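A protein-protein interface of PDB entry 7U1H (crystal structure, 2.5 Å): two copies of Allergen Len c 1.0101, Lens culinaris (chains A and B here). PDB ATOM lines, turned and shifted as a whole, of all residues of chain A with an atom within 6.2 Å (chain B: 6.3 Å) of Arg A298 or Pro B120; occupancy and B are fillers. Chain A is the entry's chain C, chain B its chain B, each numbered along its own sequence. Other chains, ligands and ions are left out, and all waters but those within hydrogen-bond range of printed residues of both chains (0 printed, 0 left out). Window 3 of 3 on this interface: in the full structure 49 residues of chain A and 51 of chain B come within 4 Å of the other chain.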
ATOM      1  N   ASP A 277      -5.853 -11.240  15.601  1.00  0.00           N
ATOM      2  CA  ASP A 277      -5.117 -10.622  14.466  1.00  0.00           C
ATOM      3  C   ASP A 277      -4.245  -9.476  14.988  1.00  0.00           C
ATOM      4  O   ASP A 277      -4.439  -8.297  14.590  1.00  0.00           O
ATOM      5  CB  ASP A 277      -6.080 -10.172  13.369  1.00  0.00           C
ATOM      6  CG  ASP A 277      -5.324  -9.766  12.127  1.00  0.00           C
ATOM      7  OD1 ASP A 277      -5.856  -8.913  11.384  1.00  0.00           O
ATOM      8  OD2 ASP A 277      -4.190 -10.277  11.950  1.00  0.00           O
ATOM      9  N   ASN A 296       4.269   1.106   9.299  1.00  0.00           N
ATOM     10  CA  ASN A 296       3.578  -0.193   9.077  1.00  0.00           C
ATOM     11  C   ASN A 296       2.561  -0.049   7.941  1.00  0.00           C
ATOM     12  O   ASN A 296       1.835   0.982   7.927  1.00  0.00           O
ATOM     13  CB  ASN A 296       2.830  -0.659  10.323  1.00  0.00           C
ATOM     14  CG  ASN A 296       3.770  -1.015  11.455  1.00  0.00           C
ATOM     15  OD1 ASN A 296       4.503  -2.007  11.385  1.00  0.00           O
ATOM     16  ND2 ASN A 296       3.742  -0.209  12.498  1.00  0.00           N
ATOM     17  N   SER A 297       2.476  -1.070   7.074  1.00  0.00           N
ATOM     18  CA  SER A 297       1.650  -1.064   5.836  1.00  0.00           C
ATOM     19  C   SER A 297       0.170  -1.007   6.219  1.00  0.00           C
ATOM     20  O   SER A 297      -0.548  -0.158   5.630  1.00  0.00           O
ATOM     21  CB  SER A 297       1.978  -2.247   4.883  1.00  0.00           C
ATOM     22  OG  SER A 297       1.601  -3.511   5.425  1.00  0.00           O
ATOM     23  N   ARG A 298      -0.223  -1.822   7.198  1.00  0.00           N
ATOM     24  CA  ARG A 298      -1.633  -2.171   7.538  1.00  0.00           C
ATOM     25  C   ARG A 298      -1.915  -1.989   9.041  1.00  0.00           C
ATOM     26  O   ARG A 298      -3.074  -1.624   9.413  1.00  0.00           O
ATOM     27  CB  ARG A 298      -1.864  -3.622   7.107  1.00  0.00           C
ATOM     28  CG  ARG A 298      -3.107  -4.258   7.702  1.00  0.00           C
ATOM     29  CD  ARG A 298      -3.297  -5.687   7.215  1.00  0.00           C
ATOM     30  NE  ARG A 298      -3.082  -5.619   5.799  1.00  0.00           N
ATOM     31  CZ  ARG A 298      -3.987  -5.219   4.917  1.00  0.00           C
ATOM     32  NH1 ARG A 298      -5.232  -4.951   5.271  1.00  0.00           N
ATOM     33  NH2 ARG A 298      -3.626  -5.119   3.654  1.00  0.00           N
ATOM     34  N   ALA A 299      -0.935  -2.277   9.900  1.00  0.00           N
ATOM     35  CA  ALA A 299      -1.178  -2.459  11.343  1.00  0.00           C
ATOM     36  C   ALA A 299      -1.186  -1.110  12.057  1.00  0.00           C
ATOM     37  O   ALA A 299      -0.340  -0.243  11.728  1.00  0.00           O
ATOM     38  CB  ALA A 299      -0.159  -3.378  11.929  1.00  0.00           C
ATOM     39  N   ILE A 300      -2.137  -0.959  12.982  1.00  0.00           N
ATOM     40  CA  ILE A 300      -2.230   0.172  13.940  1.00  0.00           C
ATOM     41  C   ILE A 300      -1.574  -0.271  15.247  1.00  0.00           C
ATOM     42  O   ILE A 300      -2.031  -1.267  15.847  1.00  0.00           O
ATOM     43  CB  ILE A 300      -3.700   0.570  14.140  1.00  0.00           C
ATOM     44  CG1 ILE A 300      -4.321   1.031  12.828  1.00  0.00           C
ATOM     45  CG2 ILE A 300      -3.840   1.627  15.233  1.00  0.00           C
ATOM     46  CD1 ILE A 300      -5.814   0.936  12.792  1.00  0.00           C
ATOM     47  N   ALA A 360      -1.762   3.047  10.817  1.00  0.00           N
ATOM     48  CA  ALA A 360      -1.166   2.479   9.593  1.00  0.00           C
ATOM     49  C   ALA A 360      -0.667   3.597   8.670  1.00  0.00           C
ATOM     50  O   ALA A 360      -1.317   4.651   8.567  1.00  0.00           O
ATOM     51  CB  ALA A 360      -2.155   1.584   8.891  1.00  0.00           C
ATOM     52  N   GLY A 361       0.480   3.350   8.036  1.00  0.00           N
ATOM     53  CA  GLY A 361       1.099   4.212   7.028  1.00  0.00           C
ATOM     54  C   GLY A 361       1.533   5.542   7.593  1.00  0.00           C
ATOM     55  O   GLY A 361       1.948   6.393   6.807  1.00  0.00           O
ATOM     56  N   ILE A 379      -2.665  -3.907  15.965  1.00  0.00           N
ATOM     57  CA  ILE A 379      -4.021  -4.327  15.486  1.00  0.00           C
ATOM     58  C   ILE A 379      -3.927  -4.438  13.953  1.00  0.00           C
ATOM     59  O   ILE A 379      -3.184  -3.640  13.380  1.00  0.00           O
ATOM     60  CB  ILE A 379      -5.112  -3.359  16.006  1.00  0.00           C
ATOM     61  CG1 ILE A 379      -5.456  -3.607  17.480  1.00  0.00           C
ATOM     62  CG2 ILE A 379      -6.388  -3.443  15.191  1.00  0.00           C
ATOM     63  CD1 ILE A 379      -4.327  -3.447  18.455  1.00  0.00           C
ATOM     64  N   ASN A 380      -4.544  -5.464  13.350  1.00  0.00           N
ATOM     65  CA  ASN A 380      -4.491  -5.813  11.898  1.00  0.00           C
ATOM     66  C   ASN A 380      -3.091  -6.279  11.492  1.00  0.00           C
ATOM     67  O   ASN A 380      -2.595  -5.784  10.472  1.00  0.00           O
ATOM     68  CB  ASN A 380      -4.856  -4.655  10.961  1.00  0.00           C
ATOM     69  CG  ASN A 380      -6.112  -3.928  11.369  1.00  0.00           C
ATOM     70  OD1 ASN A 380      -6.984  -4.483  12.041  1.00  0.00           O
ATOM     71  ND2 ASN A 380      -6.202  -2.668  10.971  1.00  0.00           N
ATOM     72  N   ALA A 381      -2.504  -7.222  12.219  1.00  0.00           N
ATOM     73  CA  ALA A 381      -1.079  -7.592  12.082  1.00  0.00           C
ATOM     74  C   ALA A 381      -0.856  -8.465  10.837  1.00  0.00           C
ATOM     75  O   ALA A 381       0.203  -8.333  10.206  1.00  0.00           O
ATOM     76  CB  ALA A 381      -0.628  -8.288  13.341  1.00  0.00           C
ATOM     77  N   LYS A 382      -1.791  -9.362  10.512  1.00  0.00           N
ATOM     78  CA  LYS A 382      -1.646 -10.312   9.368  1.00  0.00           C
ATOM     79  C   LYS A 382      -1.317  -9.494   8.107  1.00  0.00           C
ATOM     80  O   LYS A 382      -2.001  -8.474   7.858  1.00  0.00           O
ATOM     81  CB  LYS A 382      -2.910 -11.169   9.194  1.00  0.00           C
ATOM     82  CG  LYS A 382      -2.762 -12.394   8.301  1.00  0.00           C
ATOM     83  CD  LYS A 382      -4.059 -12.819   7.632  1.00  0.00           C
ATOM     84  CE  LYS A 382      -3.928 -14.086   6.802  1.00  0.00           C
ATOM     85  NZ  LYS A 382      -4.334 -13.860   5.390  1.00  0.00           N
ATOM     86  N   ASN A 383      -0.262  -9.901   7.401  1.00  0.00           N
ATOM     87  CA  ASN A 383       0.252  -9.302   6.133  1.00  0.00           C
ATOM     88  C   ASN A 383       0.823  -7.900   6.358  1.00  0.00           C
ATOM     89  O   ASN A 383       1.264  -7.299   5.379  1.00  0.00           O
ATOM     90  CB  ASN A 383      -0.799  -9.336   5.025  1.00  0.00           C
ATOM     91  CG  ASN A 383      -0.978 -10.748   4.514  1.00  0.00           C
ATOM     92  OD1 ASN A 383      -0.009 -11.481   4.342  1.00  0.00           O
ATOM     93  ND2 ASN A 383      -2.213 -11.159   4.333  1.00  0.00           N
ATOM     94  N   ASN A 384       0.921  -7.430   7.596  1.00  0.00           N
ATOM     95  CA  ASN A 384       1.577  -6.127   7.871  1.00  0.00           C
ATOM     96  C   ASN A 384       3.008  -6.162   7.312  1.00  0.00           C
ATOM     97  O   ASN A 384       3.700  -7.169   7.525  1.00  0.00           O
ATOM     98  CB  ASN A 384       1.607  -5.759   9.350  1.00  0.00           C
ATOM     99  CG  ASN A 384       2.127  -4.353   9.538  1.00  0.00           C
ATOM    100  OD1 ASN A 384       1.499  -3.397   9.100  1.00  0.00           O
ATOM    101  ND2 ASN A 384       3.279  -4.209  10.168  1.00  0.00           N
ATOM    102  N   GLN A 385       3.405  -5.117   6.588  1.00  0.00           N
ATOM    103  CA  GLN A 385       4.798  -4.892   6.145  1.00  0.00           C
ATOM    104  C   GLN A 385       5.278  -3.614   6.851  1.00  0.00           C
ATOM    105  O   GLN A 385       4.519  -2.631   6.811  1.00  0.00           O
ATOM    106  CB  GLN A 385       4.778  -4.801   4.622  1.00  0.00           C
ATOM    107  CG  GLN A 385       5.707  -5.781   3.920  1.00  0.00           C
ATOM    108  CD  GLN A 385       5.224  -7.211   4.003  1.00  0.00           C
ATOM    109  OE1 GLN A 385       4.027  -7.475   4.055  1.00  0.00           O
ATOM    110  NE2 GLN A 385       6.155  -8.153   4.038  1.00  0.00           N
ATOM    111  N   THR B  83      -1.239   4.740   0.518  1.00  0.00           N
ATOM    112  CA  THR B  83      -2.506   5.109   1.176  1.00  0.00           C
ATOM    113  C   THR B  83      -2.783   4.091   2.283  1.00  0.00           C
ATOM    114  O   THR B  83      -2.474   2.921   2.094  1.00  0.00           O
ATOM    115  CB  THR B  83      -3.576   5.189   0.086  1.00  0.00           C
ATOM    116  OG1 THR B  83      -3.101   6.251  -0.745  1.00  0.00           O
ATOM    117  CG2 THR B  83      -4.983   5.462   0.572  1.00  0.00           C
ATOM    118  N   ALA B  85      -5.124   2.260   2.857  1.00  0.00           N
ATOM    119  CA  ALA B  85      -6.310   1.599   2.260  1.00  0.00           C
ATOM    120  C   ALA B  85      -5.867   0.534   1.261  1.00  0.00           C
ATOM    121  O   ALA B  85      -4.960   0.792   0.508  1.00  0.00           O
ATOM    122  CB  ALA B  85      -7.193   2.624   1.609  1.00  0.00           C
ATOM    123  N   ASP B  86      -6.462  -0.651   1.320  1.00  0.00           N
ATOM    124  CA  ASP B  86      -6.285  -1.724   0.316  1.00  0.00           C
ATOM    125  C   ASP B  86      -6.914  -1.255  -0.988  1.00  0.00           C
ATOM    126  O   ASP B  86      -8.117  -0.958  -0.951  1.00  0.00           O
ATOM    127  CB  ASP B  86      -6.970  -2.995   0.800  1.00  0.00           C
ATOM    128  CG  ASP B  86      -6.357  -3.508   2.088  1.00  0.00           C
ATOM    129  OD1 ASP B  86      -5.119  -3.415   2.175  1.00  0.00           O
ATOM    130  OD2 ASP B  86      -7.118  -3.961   3.004  1.00  0.00           O
ATOM    131  N   PHE B  87      -6.159  -1.188  -2.088  1.00  0.00           N
ATOM    132  CA  PHE B  87      -6.705  -0.833  -3.423  1.00  0.00           C
ATOM    133  C   PHE B  87      -6.913  -2.117  -4.232  1.00  0.00           C
ATOM    134  O   PHE B  87      -6.021  -3.016  -4.204  1.00  0.00           O
ATOM    135  CB  PHE B  87      -5.798   0.148  -4.173  1.00  0.00           C
ATOM    136  CG  PHE B  87      -5.870   1.590  -3.728  1.00  0.00           C
ATOM    137  CD1 PHE B  87      -5.365   2.586  -4.528  1.00  0.00           C
ATOM    138  CD2 PHE B  87      -6.407   1.960  -2.515  1.00  0.00           C
ATOM    139  CE1 PHE B  87      -5.405   3.912  -4.133  1.00  0.00           C
ATOM    140  CE2 PHE B  87      -6.484   3.287  -2.135  1.00  0.00           C
ATOM    141  CZ  PHE B  87      -5.964   4.262  -2.934  1.00  0.00           C
ATOM    142  N   VAL B 100       5.457  -2.035  -8.117  1.00  0.00           N
ATOM    143  CA  VAL B 100       4.984  -2.316  -6.733  1.00  0.00           C
ATOM    144  C   VAL B 100       6.210  -2.569  -5.872  1.00  0.00           C
ATOM    145  O   VAL B 100       6.962  -3.478  -6.222  1.00  0.00           O
ATOM    146  CB  VAL B 100       4.027  -3.521  -6.691  1.00  0.00           C
ATOM    147  CG1 VAL B 100       3.450  -3.718  -5.288  1.00  0.00           C
ATOM    148  CG2 VAL B 100       2.921  -3.394  -7.736  1.00  0.00           C
ATOM    149  N   LYS B 118      -4.467  -6.361  -6.576  1.00  0.00           N
ATOM    150  CA  LYS B 118      -4.628  -5.840  -5.194  1.00  0.00           C
ATOM    151  C   LYS B 118      -3.305  -5.229  -4.714  1.00  0.00           C
ATOM    152  O   LYS B 118      -2.236  -5.900  -4.812  1.00  0.00           O
ATOM    153  CB  LYS B 118      -5.054  -6.924  -4.209  1.00  0.00           C
ATOM    154  CG  LYS B 118      -5.674  -6.357  -2.941  1.00  0.00           C
ATOM    155  CD  LYS B 118      -5.147  -6.918  -1.636  1.00  0.00           C
ATOM    156  CE  LYS B 118      -5.231  -8.424  -1.523  1.00  0.00           C
ATOM    157  NZ  LYS B 118      -4.848  -8.870  -0.170  1.00  0.00           N
ATOM    158  N   LEU B 119      -3.389  -3.972  -4.270  1.00  0.00           N
ATOM    159  CA  LEU B 119      -2.305  -3.187  -3.640  1.00  0.00           C
ATOM    160  C   LEU B 119      -2.688  -3.021  -2.183  1.00  0.00           C
ATOM    161  O   LEU B 119      -3.501  -2.170  -1.839  1.00  0.00           O
ATOM    162  CB  LEU B 119      -2.149  -1.820  -4.311  1.00  0.00           C
ATOM    163  CG  LEU B 119      -1.594  -1.871  -5.732  1.00  0.00           C
ATOM    164  CD1 LEU B 119      -2.712  -2.115  -6.733  1.00  0.00           C
ATOM    165  CD2 LEU B 119      -0.837  -0.601  -6.093  1.00  0.00           C
ATOM    166  N   PRO B 120      -2.130  -3.872  -1.312  1.00  0.00           N
ATOM    167  CA  PRO B 120      -2.344  -3.747   0.125  1.00  0.00           C
ATOM    168  C   PRO B 120      -2.067  -2.316   0.587  1.00  0.00           C
ATOM    169  O   PRO B 120      -1.192  -1.715   0.032  1.00  0.00           O
ATOM    170  CB  PRO B 120      -1.313  -4.726   0.681  1.00  0.00           C
ATOM    171  CG  PRO B 120      -1.215  -5.802  -0.392  1.00  0.00           C
ATOM    172  CD  PRO B 120      -1.300  -5.032  -1.685  1.00  0.00           C
ATOM    173  N   ALA B 121      -2.831  -1.800   1.549  1.00  0.00           N
ATOM    174  CA  ALA B 121      -2.555  -0.508   2.214  1.00  0.00           C
ATOM    175  C   ALA B 121      -1.054  -0.385   2.473  1.00  0.00           C
ATOM    176  O   ALA B 121      -0.409  -1.393   2.736  1.00  0.00           O
ATOM    177  CB  ALA B 121      -3.322  -0.380   3.503  1.00  0.00           C
ATOM    178  N   GLY B 122      -0.548   0.839   2.393  1.00  0.00           N
ATOM    179  CA  GLY B 122       0.839   1.202   2.741  1.00  0.00           C
ATOM    180  C   GLY B 122       1.871   0.698   1.750  1.00  0.00           C
ATOM    181  O   GLY B 122       3.050   0.840   2.071  1.00  0.00           O
ATOM    182  N   THR B 123       1.462   0.159   0.599  1.00  0.00           N
ATOM    183  CA  THR B 123       2.372  -0.339  -0.461  1.00  0.00           C
ATOM    184  C   THR B 123       2.697   0.800  -1.431  1.00  0.00           C
ATOM    185  O   THR B 123       1.764   1.276  -2.066  1.00  0.00           O
ATOM    186  CB  THR B 123       1.776  -1.508  -1.252  1.00  0.00           C
ATOM    187  OG1 THR B 123       0.947  -2.261  -0.383  1.00  0.00           O
ATOM    188  CG2 THR B 123       2.822  -2.448  -1.803  1.00  0.00           C
ATOM    189  N   ILE B 124       3.983   1.180  -1.568  1.00  0.00           N
ATOM    190  CA  ILE B 124       4.440   2.207  -2.552  1.00  0.00           C
ATOM    191  C   ILE B 124       4.304   1.636  -3.965  1.00  0.00           C
ATOM    192  O   ILE B 124       4.904   0.571  -4.261  1.00  0.00           O
ATOM    193  CB  ILE B 124       5.869   2.715  -2.290  1.00  0.00           C
ATOM    194  CG1 ILE B 124       6.100   3.086  -0.818  1.00  0.00           C
ATOM    195  CG2 ILE B 124       6.185   3.857  -3.250  1.00  0.00           C
ATOM    196  CD1 ILE B 124       6.600   4.487  -0.552  1.00  0.00           C
ATOM    197  N   VAL B 145      -8.090   1.218   6.056  1.00  0.00           N
ATOM    198  CA  VAL B 145      -7.702   0.422   7.246  1.00  0.00           C
ATOM    199  C   VAL B 145      -7.708   1.301   8.509  1.00  0.00           C
ATOM    200  O   VAL B 145      -7.986   0.745   9.569  1.00  0.00           O
ATOM    201  CB  VAL B 145      -6.377  -0.305   7.001  1.00  0.00           C
ATOM    202  CG1 VAL B 145      -5.385   0.504   6.203  1.00  0.00           C
ATOM    203  CG2 VAL B 145      -5.759  -0.733   8.300  1.00  0.00           C
ATOM    204  N   ASN B 146      -7.519   2.623   8.425  1.00  0.00           N
ATOM    205  CA  ASN B 146      -7.373   3.468   9.648  1.00  0.00           C
ATOM    206  C   ASN B 146      -8.766   3.860  10.144  1.00  0.00           C
ATOM    207  O   ASN B 146      -9.213   3.204  11.059  1.00  0.00           O
ATOM    208  CB  ASN B 146      -6.430   4.666   9.467  1.00  0.00           C
ATOM    209  CG  ASN B 146      -4.969   4.286   9.574  1.00  0.00           C
ATOM    210  OD1 ASN B 146      -4.558   3.635  10.539  1.00  0.00           O
ATOM    211  ND2 ASN B 146      -4.169   4.710   8.608  1.00  0.00           N
ATOM    212  N   LEU B 276     -10.638  -9.864   1.554  1.00  0.00           N
ATOM    213  CA  LEU B 276     -11.586  -8.721   1.421  1.00  0.00           C
ATOM    214  C   LEU B 276     -12.979  -9.201   0.976  1.00  0.00           C
ATOM    215  O   LEU B 276     -13.924  -8.388   1.055  1.00  0.00           O
ATOM    216  CB  LEU B 276     -11.027  -7.708   0.429  1.00  0.00           C
ATOM    217  CG  LEU B 276      -9.809  -6.941   0.921  1.00  0.00           C
ATOM    218  CD1 LEU B 276      -8.814  -6.757  -0.213  1.00  0.00           C
ATOM    219  CD2 LEU B 276     -10.227  -5.601   1.524  1.00  0.00           C
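The side-chain carboxylate (OD1) of Asp B86 lies within salt-bridge range of the guanidinium group (NH2) of Arg A298 (2.7 Å). The backbone NH (N) of Gly B122 lies within hydrogen-bond range of the backbone carbonyl oxygen (O) of Ser A297 (3.4 Å). The side-chain amide nitrogen of Asn B146 is in hydrogen-bond range of the backbone carbonyl oxygen of Ala A360. O of Ser A297 sits close to O of Ala B121 (3.1 Å).
The backbone carbonyl oxygen (O) of Thr B83 is in hydrogen-bond range of the backbone NH (N) of Gly B122 (2.9 Å). The side-chain carboxylate (OD1) of Asp B86 sits at hydrogen-bond distance from the backbone NH (N) of Ala B121 (2.9 Å). The backbone carbonyl oxygen of Asp A277 is in hydrogen-bond range of the backbone NH of Asn A380 (3.1 Å). The side-chain amide oxygen of Asn A384 is in hydrogen-bond range of the backbone NH of Ser A297 (3.2 Å). N of Ser A297 is in hydrogen-bond range of O of Gln A385 (2.6 Å). O of Ile A300 is in hydrogen-bond range of N of Ile A379 (2.7 Å).
Among the printed residues, merely in contact across the chains: Arg A298 with Pro B120, Arg A298 with Val B145, Ile A300 with Val B145, Ile A300 with Asn B146 and Asn A380 with Val B145.
Printed residues of chain B within 4 Å of Ser A297: Ala B121 (3.1 Å) and Gly B122 (3.4 Å). Printed residues of chain B within 4 Å of Arg A298: Asp B86, Pro B120 and Val B145. Of the printed residues of chain B, Ile A300 touches Val B145 (3.9 Å) and Asn B146 (3.5 Å). Printed residues of chain B within 4 Å of Asn A380: Val B145. Of chain A, only Arg A298 comes within 4 Å of Pro B120. Of the printed residues of chain A, Ala B121 touches Ser A297. Of the printed residues of chain A, Val B145 touches Arg A298, Ile A300 and Asn A380.
Hydrophobic or aromatic side chains of chain A that line the printed part of chain B: Ile A300 and Ala A360. Among the printed residues, 9 pairs touch across the chains.
No position is printed for both chains. Of the 9 pairs that touch across the chains among the printed residues, none has its exchanged pair printed and touching as well.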
